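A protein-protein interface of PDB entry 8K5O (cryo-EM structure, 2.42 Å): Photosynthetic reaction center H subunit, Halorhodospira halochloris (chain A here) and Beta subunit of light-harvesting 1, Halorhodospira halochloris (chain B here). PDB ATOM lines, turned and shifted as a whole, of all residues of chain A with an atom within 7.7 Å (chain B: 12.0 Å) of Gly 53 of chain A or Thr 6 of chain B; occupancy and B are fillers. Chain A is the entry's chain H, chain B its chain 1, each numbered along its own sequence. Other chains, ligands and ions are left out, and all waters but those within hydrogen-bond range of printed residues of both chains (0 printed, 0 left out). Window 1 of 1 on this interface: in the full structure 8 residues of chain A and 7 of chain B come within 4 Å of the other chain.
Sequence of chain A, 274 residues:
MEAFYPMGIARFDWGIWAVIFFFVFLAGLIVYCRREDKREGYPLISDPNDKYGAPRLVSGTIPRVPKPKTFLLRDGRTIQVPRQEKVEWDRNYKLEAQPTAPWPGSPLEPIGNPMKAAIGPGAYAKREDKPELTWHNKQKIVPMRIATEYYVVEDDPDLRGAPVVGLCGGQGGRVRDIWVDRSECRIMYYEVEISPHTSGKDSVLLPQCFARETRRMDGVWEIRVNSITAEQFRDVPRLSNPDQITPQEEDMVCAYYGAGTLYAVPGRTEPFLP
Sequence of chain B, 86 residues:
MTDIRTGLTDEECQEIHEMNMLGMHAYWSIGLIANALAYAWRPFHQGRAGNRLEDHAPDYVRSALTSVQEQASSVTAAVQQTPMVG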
ATOM      1  N   SER A  46      31.055  23.113 -11.981  1.00  0.00           N
ATOM      2  CA  SER A  46      30.598  23.394 -10.632  1.00  0.00           C
ATOM      3  C   SER A  46      30.574  22.109  -9.810  1.00  0.00           C
ATOM      4  O   SER A  46      30.700  21.002 -10.335  1.00  0.00           O
ATOM      5  CB  SER A  46      29.218  24.044 -10.662  1.00  0.00           C
ATOM      6  OG  SER A  46      28.251  23.168 -11.203  1.00  0.00           O
ATOM      7  N   ASP A  47      30.441  22.268  -8.503  1.00  0.00           N
ATOM      8  CA  ASP A  47      30.344  21.114  -7.623  1.00  0.00           C
ATOM      9  C   ASP A  47      28.995  20.435  -7.818  1.00  0.00           C
ATOM     10  O   ASP A  47      27.955  21.078  -7.621  1.00  0.00           O
ATOM     11  CB  ASP A  47      30.518  21.534  -6.165  1.00  0.00           C
ATOM     12  CG  ASP A  47      30.864  20.371  -5.252  1.00  0.00           C
ATOM     13  OD1 ASP A  47      30.377  19.249  -5.492  1.00  0.00           O
ATOM     14  OD2 ASP A  47      31.621  20.580  -4.281  1.00  0.00           O
ATOM     15  N   PRO A  48      28.961  19.158  -8.205  1.00  0.00           N
ATOM     16  CA  PRO A  48      27.673  18.456  -8.290  1.00  0.00           C
ATOM     17  C   PRO A  48      26.936  18.412  -6.969  1.00  0.00           C
ATOM     18  O   PRO A  48      25.699  18.400  -6.958  1.00  0.00           O
ATOM     19  CB  PRO A  48      28.070  17.053  -8.763  1.00  0.00           C
ATOM     20  CG  PRO A  48      29.377  17.237  -9.434  1.00  0.00           C
ATOM     21  CD  PRO A  48      30.074  18.335  -8.701  1.00  0.00           C
ATOM     22  N   ASP A  50      25.213  20.057  -4.685  1.00  0.00           N
ATOM     23  CA  ASP A  50      24.615  21.383  -4.705  1.00  0.00           C
ATOM     24  C   ASP A  50      23.110  21.217  -4.792  1.00  0.00           C
ATOM     25  O   ASP A  50      22.618  20.485  -5.654  1.00  0.00           O
ATOM     26  CB  ASP A  50      25.140  22.195  -5.895  1.00  0.00           C
ATOM     27  CG  ASP A  50      24.728  23.649  -5.842  1.00  0.00           C
ATOM     28  OD1 ASP A  50      24.082  24.052  -4.857  1.00  0.00           O
ATOM     29  OD2 ASP A  50      25.056  24.390  -6.791  1.00  0.00           O
ATOM     30  N   LYS A  51      22.385  21.891  -3.902  1.00  0.00           N
ATOM     31  CA  LYS A  51      20.932  21.845  -3.957  1.00  0.00           C
ATOM     32  C   LYS A  51      20.373  22.604  -5.149  1.00  0.00           C
ATOM     33  O   LYS A  51      19.185  22.459  -5.452  1.00  0.00           O
ATOM     34  CB  LYS A  51      20.334  22.397  -2.666  1.00  0.00           C
ATOM     35  CG  LYS A  51      20.759  21.640  -1.426  1.00  0.00           C
ATOM     36  CD  LYS A  51      20.009  22.132  -0.216  1.00  0.00           C
ATOM     37  CE  LYS A  51      20.475  21.446   1.045  1.00  0.00           C
ATOM     38  NZ  LYS A  51      21.836  21.902   1.424  1.00  0.00           N
ATOM     39  N   TYR A  52      21.194  23.396  -5.829  1.00  0.00           N
ATOM     40  CA  TYR A  52      20.775  24.155  -6.993  1.00  0.00           C
ATOM     41  C   TYR A  52      21.501  23.656  -8.233  1.00  0.00           C
ATOM     42  O   TYR A  52      22.549  23.011  -8.152  1.00  0.00           O
ATOM     43  CB  TYR A  52      21.026  25.652  -6.791  1.00  0.00           C
ATOM     44  CG  TYR A  52      20.147  26.254  -5.723  1.00  0.00           C
ATOM     45  CD1 TYR A  52      20.546  26.275  -4.396  1.00  0.00           C
ATOM     46  CD2 TYR A  52      18.911  26.790  -6.043  1.00  0.00           C
ATOM     47  CE1 TYR A  52      19.739  26.813  -3.421  1.00  0.00           C
ATOM     48  CE2 TYR A  52      18.099  27.336  -5.077  1.00  0.00           C
ATOM     49  CZ  TYR A  52      18.518  27.349  -3.767  1.00  0.00           C
ATOM     50  OH  TYR A  52      17.708  27.893  -2.802  1.00  0.00           O
ATOM     51  N   GLY A  53      20.929  23.965  -9.388  1.00  0.00           N
ATOM     52  CA  GLY A  53      21.494  23.537 -10.645  1.00  0.00           C
ATOM     53  C   GLY A  53      22.757  24.300 -10.985  1.00  0.00           C
ATOM     54  O   GLY A  53      23.244  25.150 -10.240  1.00  0.00           O
ATOM     55  N   ALA A  54      23.302  23.969 -12.126  1.00  0.00           N
ATOM     56  CA  ALA A  54      24.498  24.642 -12.611  1.00  0.00           C
ATOM     57  C   ALA A  54      24.114  25.895 -13.383  1.00  0.00           C
ATOM     58  O   ALA A  54      23.247  25.831 -14.262  1.00  0.00           O
ATOM     59  CB  ALA A  54      25.316  23.721 -13.504  1.00  0.00           C
ATOM     60  N   PRO A  55      24.711  27.044 -13.079  1.00  0.00           N
ATOM     61  CA  PRO A  55      24.497  28.222 -13.923  1.00  0.00           C
ATOM     62  C   PRO A  55      24.976  27.949 -15.340  1.00  0.00           C
ATOM     63  O   PRO A  55      25.931  27.203 -15.562  1.00  0.00           O
ATOM     64  CB  PRO A  55      25.335  29.311 -13.243  1.00  0.00           C
ATOM     65  CG  PRO A  55      25.597  28.802 -11.874  1.00  0.00           C
ATOM     66  CD  PRO A  55      25.609  27.320 -11.949  1.00  0.00           C
ATOM     67  N   ARG A  56      24.282  28.552 -16.306  1.00  0.00           N
ATOM     68  CA  ARG A  56      24.602  28.305 -17.708  1.00  0.00           C
ATOM     69  C   ARG A  56      26.028  28.722 -18.029  1.00  0.00           C
ATOM     70  O   ARG A  56      26.737  28.025 -18.764  1.00  0.00           O
ATOM     71  CB  ARG A  56      23.607  29.038 -18.605  1.00  0.00           C
ATOM     72  CG  ARG A  56      23.764  28.759 -20.080  1.00  0.00           C
ATOM     73  CD  ARG A  56      23.710  27.278 -20.380  1.00  0.00           C
ATOM     74  NE  ARG A  56      23.901  27.018 -21.801  1.00  0.00           N
ATOM     75  CZ  ARG A  56      25.072  27.065 -22.420  1.00  0.00           C
ATOM     76  NH1 ARG A  56      26.188  27.353 -21.771  1.00  0.00           N
ATOM     77  NH2 ARG A  56      25.125  26.818 -23.724  1.00  0.00           N
ATOM     78  N   ILE B   4      23.992  19.220 -10.544  1.00  0.00           N
ATOM     79  CA  ILE B   4      24.340  20.199 -11.565  1.00  0.00           C
ATOM     80  C   ILE B   4      24.243  19.597 -12.954  1.00  0.00           C
ATOM     81  O   ILE B   4      24.563  20.255 -13.944  1.00  0.00           O
ATOM     82  CB  ILE B   4      25.743  20.749 -11.356  1.00  0.00           C
ATOM     83  CG1 ILE B   4      26.752  19.613 -11.534  1.00  0.00           C
ATOM     84  CG2 ILE B   4      25.842  21.430  -9.996  1.00  0.00           C
ATOM     85  CD1 ILE B   4      28.160  20.062 -11.770  1.00  0.00           C
ATOM     86  N   ARG B   5      23.818  18.336 -13.032  1.00  0.00           N
ATOM     87  CA  ARG B   5      23.622  17.718 -14.337  1.00  0.00           C
ATOM     88  C   ARG B   5      22.520  18.419 -15.119  1.00  0.00           C
ATOM     89  O   ARG B   5      22.426  18.244 -16.340  1.00  0.00           O
ATOM     90  CB  ARG B   5      23.330  16.227 -14.165  1.00  0.00           C
ATOM     91  CG  ARG B   5      24.485  15.485 -13.502  1.00  0.00           C
ATOM     92  CD  ARG B   5      24.290  13.973 -13.453  1.00  0.00           C
ATOM     93  NE  ARG B   5      25.546  13.300 -13.136  1.00  0.00           N
ATOM     94  CZ  ARG B   5      25.691  11.988 -13.007  1.00  0.00           C
ATOM     95  NH1 ARG B   5      24.673  11.160 -13.167  1.00  0.00           N
ATOM     96  NH2 ARG B   5      26.890  11.495 -12.712  1.00  0.00           N
ATOM     97  N   THR B   6      21.694  19.210 -14.441  1.00  0.00           N
ATOM     98  CA  THR B   6      20.773  20.142 -15.066  1.00  0.00           C
ATOM     99  C   THR B   6      21.036  21.542 -14.522  1.00  0.00           C
ATOM    100  O   THR B   6      21.585  21.708 -13.429  1.00  0.00           O
ATOM    101  CB  THR B   6      19.314  19.742 -14.816  1.00  0.00           C
ATOM    102  OG1 THR B   6      18.441  20.616 -15.543  1.00  0.00           O
ATOM    103  CG2 THR B   6      18.984  19.817 -13.338  1.00  0.00           C
ATOM    104  N   GLY B   7      20.661  22.548 -15.302  1.00  0.00           N
ATOM    105  CA  GLY B   7      20.795  23.917 -14.859  1.00  0.00           C
ATOM    106  C   GLY B   7      19.722  24.298 -13.859  1.00  0.00           C
ATOM    107  O   GLY B   7      18.864  23.501 -13.480  1.00  0.00           O
ATOM    108  N   LEU B   8      19.780  25.552 -13.415  1.00  0.00           N
ATOM    109  CA  LEU B   8      18.774  26.051 -12.488  1.00  0.00           C
ATOM    110  C   LEU B   8      17.404  26.050 -13.146  1.00  0.00           C
ATOM    111  O   LEU B   8      17.248  26.497 -14.285  1.00  0.00           O
ATOM    112  CB  LEU B   8      19.097  27.467 -12.014  1.00  0.00           C
ATOM    113  CG  LEU B   8      20.166  27.703 -10.951  1.00  0.00           C
ATOM    114  CD1 LEU B   8      21.556  27.470 -11.502  1.00  0.00           C
ATOM    115  CD2 LEU B   8      20.027  29.081 -10.358  1.00  0.00           C
ATOM    116  N   THR B   9      16.411  25.552 -12.425  1.00  0.00           N
ATOM    117  CA  THR B   9      15.042  25.672 -12.885  1.00  0.00           C
ATOM    118  C   THR B   9      14.547  27.094 -12.656  1.00  0.00           C
ATOM    119  O   THR B   9      15.157  27.882 -11.930  1.00  0.00           O
ATOM    120  CB  THR B   9      14.146  24.669 -12.164  1.00  0.00           C
ATOM    121  OG1 THR B   9      13.825  25.165 -10.860  1.00  0.00           O
ATOM    122  CG2 THR B   9      14.859  23.339 -12.023  1.00  0.00           C
ATOM    123  N   ASP B  10      13.431  27.430 -13.305  1.00  0.00           N
ATOM    124  CA  ASP B  10      12.822  28.730 -13.061  1.00  0.00           C
ATOM    125  C   ASP B  10      12.409  28.864 -11.603  1.00  0.00           C
ATOM    126  O   ASP B  10      12.471  29.955 -11.031  1.00  0.00           O
ATOM    127  CB  ASP B  10      11.624  28.943 -13.983  1.00  0.00           C
ATOM    128  CG  ASP B  10      12.032  29.140 -15.425  1.00  0.00           C
ATOM    129  OD1 ASP B  10      13.152  29.635 -15.664  1.00  0.00           O
ATOM    130  OD2 ASP B  10      11.229  28.808 -16.321  1.00  0.00           O
ATOM    131  N   GLU B  11      11.991  27.759 -10.983  1.00  0.00           N
ATOM    132  CA  GLU B  11      11.658  27.782  -9.564  1.00  0.00           C
ATOM    133  C   GLU B  11      12.898  28.000  -8.705  1.00  0.00           C
ATOM    134  O   GLU B  11      12.889  28.816  -7.777  1.00  0.00           O
ATOM    135  CB  GLU B  11      10.948  26.485  -9.177  1.00  0.00           C
ATOM    136  CG  GLU B  11      10.531  26.431  -7.722  1.00  0.00           C
ATOM    137  CD  GLU B  11       9.482  27.466  -7.377  1.00  0.00           C
ATOM    138  OE1 GLU B  11       8.715  27.867  -8.279  1.00  0.00           O
ATOM    139  OE2 GLU B  11       9.427  27.886  -6.202  1.00  0.00           O
ATOM    140  N   GLU B  12      13.978  27.270  -8.996  1.00  0.00           N
ATOM    141  CA  GLU B  12      15.214  27.439  -8.240  1.00  0.00           C
ATOM    142  C   GLU B  12      15.772  28.843  -8.416  1.00  0.00           C
ATOM    143  O   GLU B  12      16.191  29.489  -7.447  1.00  0.00           O
ATOM    144  CB  GLU B  12      16.243  26.403  -8.688  1.00  0.00           C
ATOM    145  CG  GLU B  12      16.286  25.142  -7.853  1.00  0.00           C
ATOM    146  CD  GLU B  12      17.140  24.063  -8.488  1.00  0.00           C
ATOM    147  OE1 GLU B  12      18.248  24.384  -8.963  1.00  0.00           O
ATOM    148  OE2 GLU B  12      16.702  22.895  -8.517  1.00  0.00           O
ATOM    149  N   CYS B  13      15.770  29.336  -9.652  1.00  0.00           N
ATOM    150  CA  CYS B  13      16.285  30.669  -9.926  1.00  0.00           C
ATOM    151  C   CYS B  13      15.408  31.731  -9.277  1.00  0.00           C
ATOM    152  O   CYS B  13      15.911  32.736  -8.766  1.00  0.00           O
ATOM    153  CB  CYS B  13      16.377  30.869 -11.438  1.00  0.00           C
ATOM    154  SG  CYS B  13      17.499  32.149 -11.974  1.00  0.00           S
ATOM    155  N   GLN B  14      14.092  31.509  -9.262  1.00  0.00           N
ATOM    156  CA  GLN B  14      13.173  32.449  -8.632  1.00  0.00           C
ATOM    157  C   GLN B  14      13.357  32.485  -7.122  1.00  0.00           C
ATOM    158  O   GLN B  14      13.276  33.552  -6.509  1.00  0.00           O
ATOM    159  CB  GLN B  14      11.732  32.085  -8.984  1.00  0.00           C
ATOM    160  CG  GLN B  14      11.170  32.851 -10.166  1.00  0.00           C
ATOM    161  CD  GLN B  14      10.050  32.107 -10.854  1.00  0.00           C
ATOM    162  OE1 GLN B  14       9.605  31.061 -10.382  1.00  0.00           O
ATOM    163  NE2 GLN B  14       9.586  32.640 -11.975  1.00  0.00           N
ATOM    164  N   GLU B  15      13.585  31.329  -6.496  1.00  0.00           N
ATOM    165  CA  GLU B  15      13.781  31.347  -5.051  1.00  0.00           C
ATOM    166  C   GLU B  15      15.148  31.903  -4.686  1.00  0.00           C
ATOM    167  O   GLU B  15      15.307  32.480  -3.605  1.00  0.00           O
ATOM    168  CB  GLU B  15      13.583  29.957  -4.445  1.00  0.00           C
ATOM    169  CG  GLU B  15      14.656  28.940  -4.748  1.00  0.00           C
ATOM    170  CD  GLU B  15      14.334  27.584  -4.149  1.00  0.00           C
ATOM    171  OE1 GLU B  15      13.260  27.453  -3.524  1.00  0.00           O
ATOM    172  OE2 GLU B  15      15.150  26.651  -4.293  1.00  0.00           O
ATOM    173  N   ILE B  16      16.142  31.752  -5.564  1.00  0.00           N
ATOM    174  CA  ILE B  16      17.396  32.468  -5.354  1.00  0.00           C
ATOM    175  C   ILE B  16      17.176  33.969  -5.466  1.00  0.00           C
ATOM    176  O   ILE B  16      17.690  34.743  -4.655  1.00  0.00           O
ATOM    177  CB  ILE B  16      18.486  31.986  -6.326  1.00  0.00           C
ATOM    178  CG1 ILE B  16      18.961  30.588  -5.948  1.00  0.00           C
ATOM    179  CG2 ILE B  16      19.657  32.942  -6.326  1.00  0.00           C
ATOM    180  CD1 ILE B  16      19.956  30.012  -6.914  1.00  0.00           C
ATOM    181  N   HIS B  17      16.405  34.405  -6.463  1.00  0.00           N
ATOM    182  CA  HIS B  17      16.210  35.834  -6.665  1.00  0.00           C
ATOM    183  C   HIS B  17      15.341  36.453  -5.582  1.00  0.00           C
ATOM    184  O   HIS B  17      15.464  37.647  -5.314  1.00  0.00           O
ATOM    185  CB  HIS B  17      15.597  36.106  -8.031  1.00  0.00           C
ATOM    186  CG  HIS B  17      15.725  37.531  -8.467  1.00  0.00           C
ATOM    187  ND1 HIS B  17      14.635  38.335  -8.718  1.00  0.00           N
ATOM    188  CD2 HIS B  17      16.818  38.296  -8.696  1.00  0.00           C
ATOM    189  CE1 HIS B  17      15.051  39.531  -9.092  1.00  0.00           C
ATOM    190  NE2 HIS B  17      16.371  39.533  -9.086  1.00  0.00           N
ATOM    191  N   MET B  19      15.556  35.743  -2.342  1.00  0.00           N
ATOM    192  CA  MET B  19      16.550  36.073  -1.329  1.00  0.00           C
ATOM    193  C   MET B  19      17.481  37.171  -1.812  1.00  0.00           C
ATOM    194  O   MET B  19      17.906  38.024  -1.031  1.00  0.00           O
ATOM    195  CB  MET B  19      17.357  34.834  -0.975  1.00  0.00           C
ATOM    196  CG  MET B  19      16.543  33.714  -0.414  1.00  0.00           C
ATOM    197  SD  MET B  19      17.625  32.330  -0.115  1.00  0.00           S
ATOM    198  CE  MET B  19      17.987  31.827  -1.791  1.00  0.00           C
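Of the 15 printed residues of chain B, 7 touch a printed residue of chain A. Printed residues of chain B that touch a printed residue of chain A: Ile 4, Thr 6, Gly 7, Leu 8, Glu 12, Glu 15 and Ile 16. Of the 10 printed residues of chain A, 8 touch a printed residue of chain B. Hydrophobic or aromatic side chains of chain A that line the printed part of chain B: Pro 48, Tyr 52 and Ala 54. Along chain A the printed residues that touch a printed residue of chain B span positions 46 to 55. Among the printed residues, 16 pairs touch across the chains.
The side-chain hydroxyl (OH) of Tyr 52 of chain A lies close to the side-chain carboxylate (OE2) of Glu 15 of chain B, at 3.2 Å. The backbone NH (N) of Gly 53 of chain A is in hydrogen-bond range of the side-chain carboxylate (OE1) of Glu 12 of chain B (2.7 Å). The backbone carbonyl oxygen (O) of Thr 6 of chain B lies within hydrogen-bond range of the backbone NH (N) of Ala 54 of chain A (3.1 Å).
Of the printed residues of chain B, Gly 53 of chain A touches Thr 6 (3.3 Å), Gly 7 (3.7 Å), Leu 8 (3.1 Å) and Glu 12 (2.7 Å). Printed residues of chain A within 4 Å of Thr 6 of chain B: Gly 53 (3.3 Å) and Ala 54 (3.1 Å). Asp 50 of chain A touches none of the printed residues of chain B. Ala 54 of chain A touches four residues of chain B. Of the printed residues of chain B, Pro 55 of chain A touches Leu 8. Of the printed residues of chain B, Tyr 52 of chain A touches Glu 12 (3.2 Å), Glu 15 (3.1 Å) and Ile 16 (3.5 Å). Of the printed residues of chain B, Lys 51 of chain A touches Glu 12 (3.97 Å). The nearest residue of chain B that does not touch Gly 53 of chain A is Ile 4 of chain B (4.3 Å).
CD1 of Ile 4 of chain B touches O of Ser 46 of chain A (3.1 Å). Asp 47 of chain A touches Ile 4 of chain B (O to CG2, 3.2 Å). O of Lys 51 of chain A touches OE2 of Glu 12 of chain B, 3.97 Å away. Ile 16 of chain B touches Tyr 52 of chain A (CG1 to CE2, 3.5 Å). Gly 53 of chain A touches Thr 6 of chain B (CA to O, 3.3 Å). CA of Gly 53 of chain A touches C of Gly 7 of chain B (3.7 Å). O of Gly 53 of chain A touches CD1 of Leu 8 of chain B, 3.1 Å away. CB of Ala 54 of chain A touches O of Ile 4 of chain B, 3.6 Å away. Ala 54 of chain A touches Gly 7 of chain B. Leu 8 of chain B touches Ala 54 of chain A.
The side-chain carboxylate (OD1) of Asp 50 of chain A sits close to the backbone NH (N) of Tyr 52 of chain A (3.1 Å). The side-chain hydroxyl of Thr 9 of chain B lies within hydrogen-bond range of the backbone NH of Glu 12 of chain B, 2.8 Å away.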
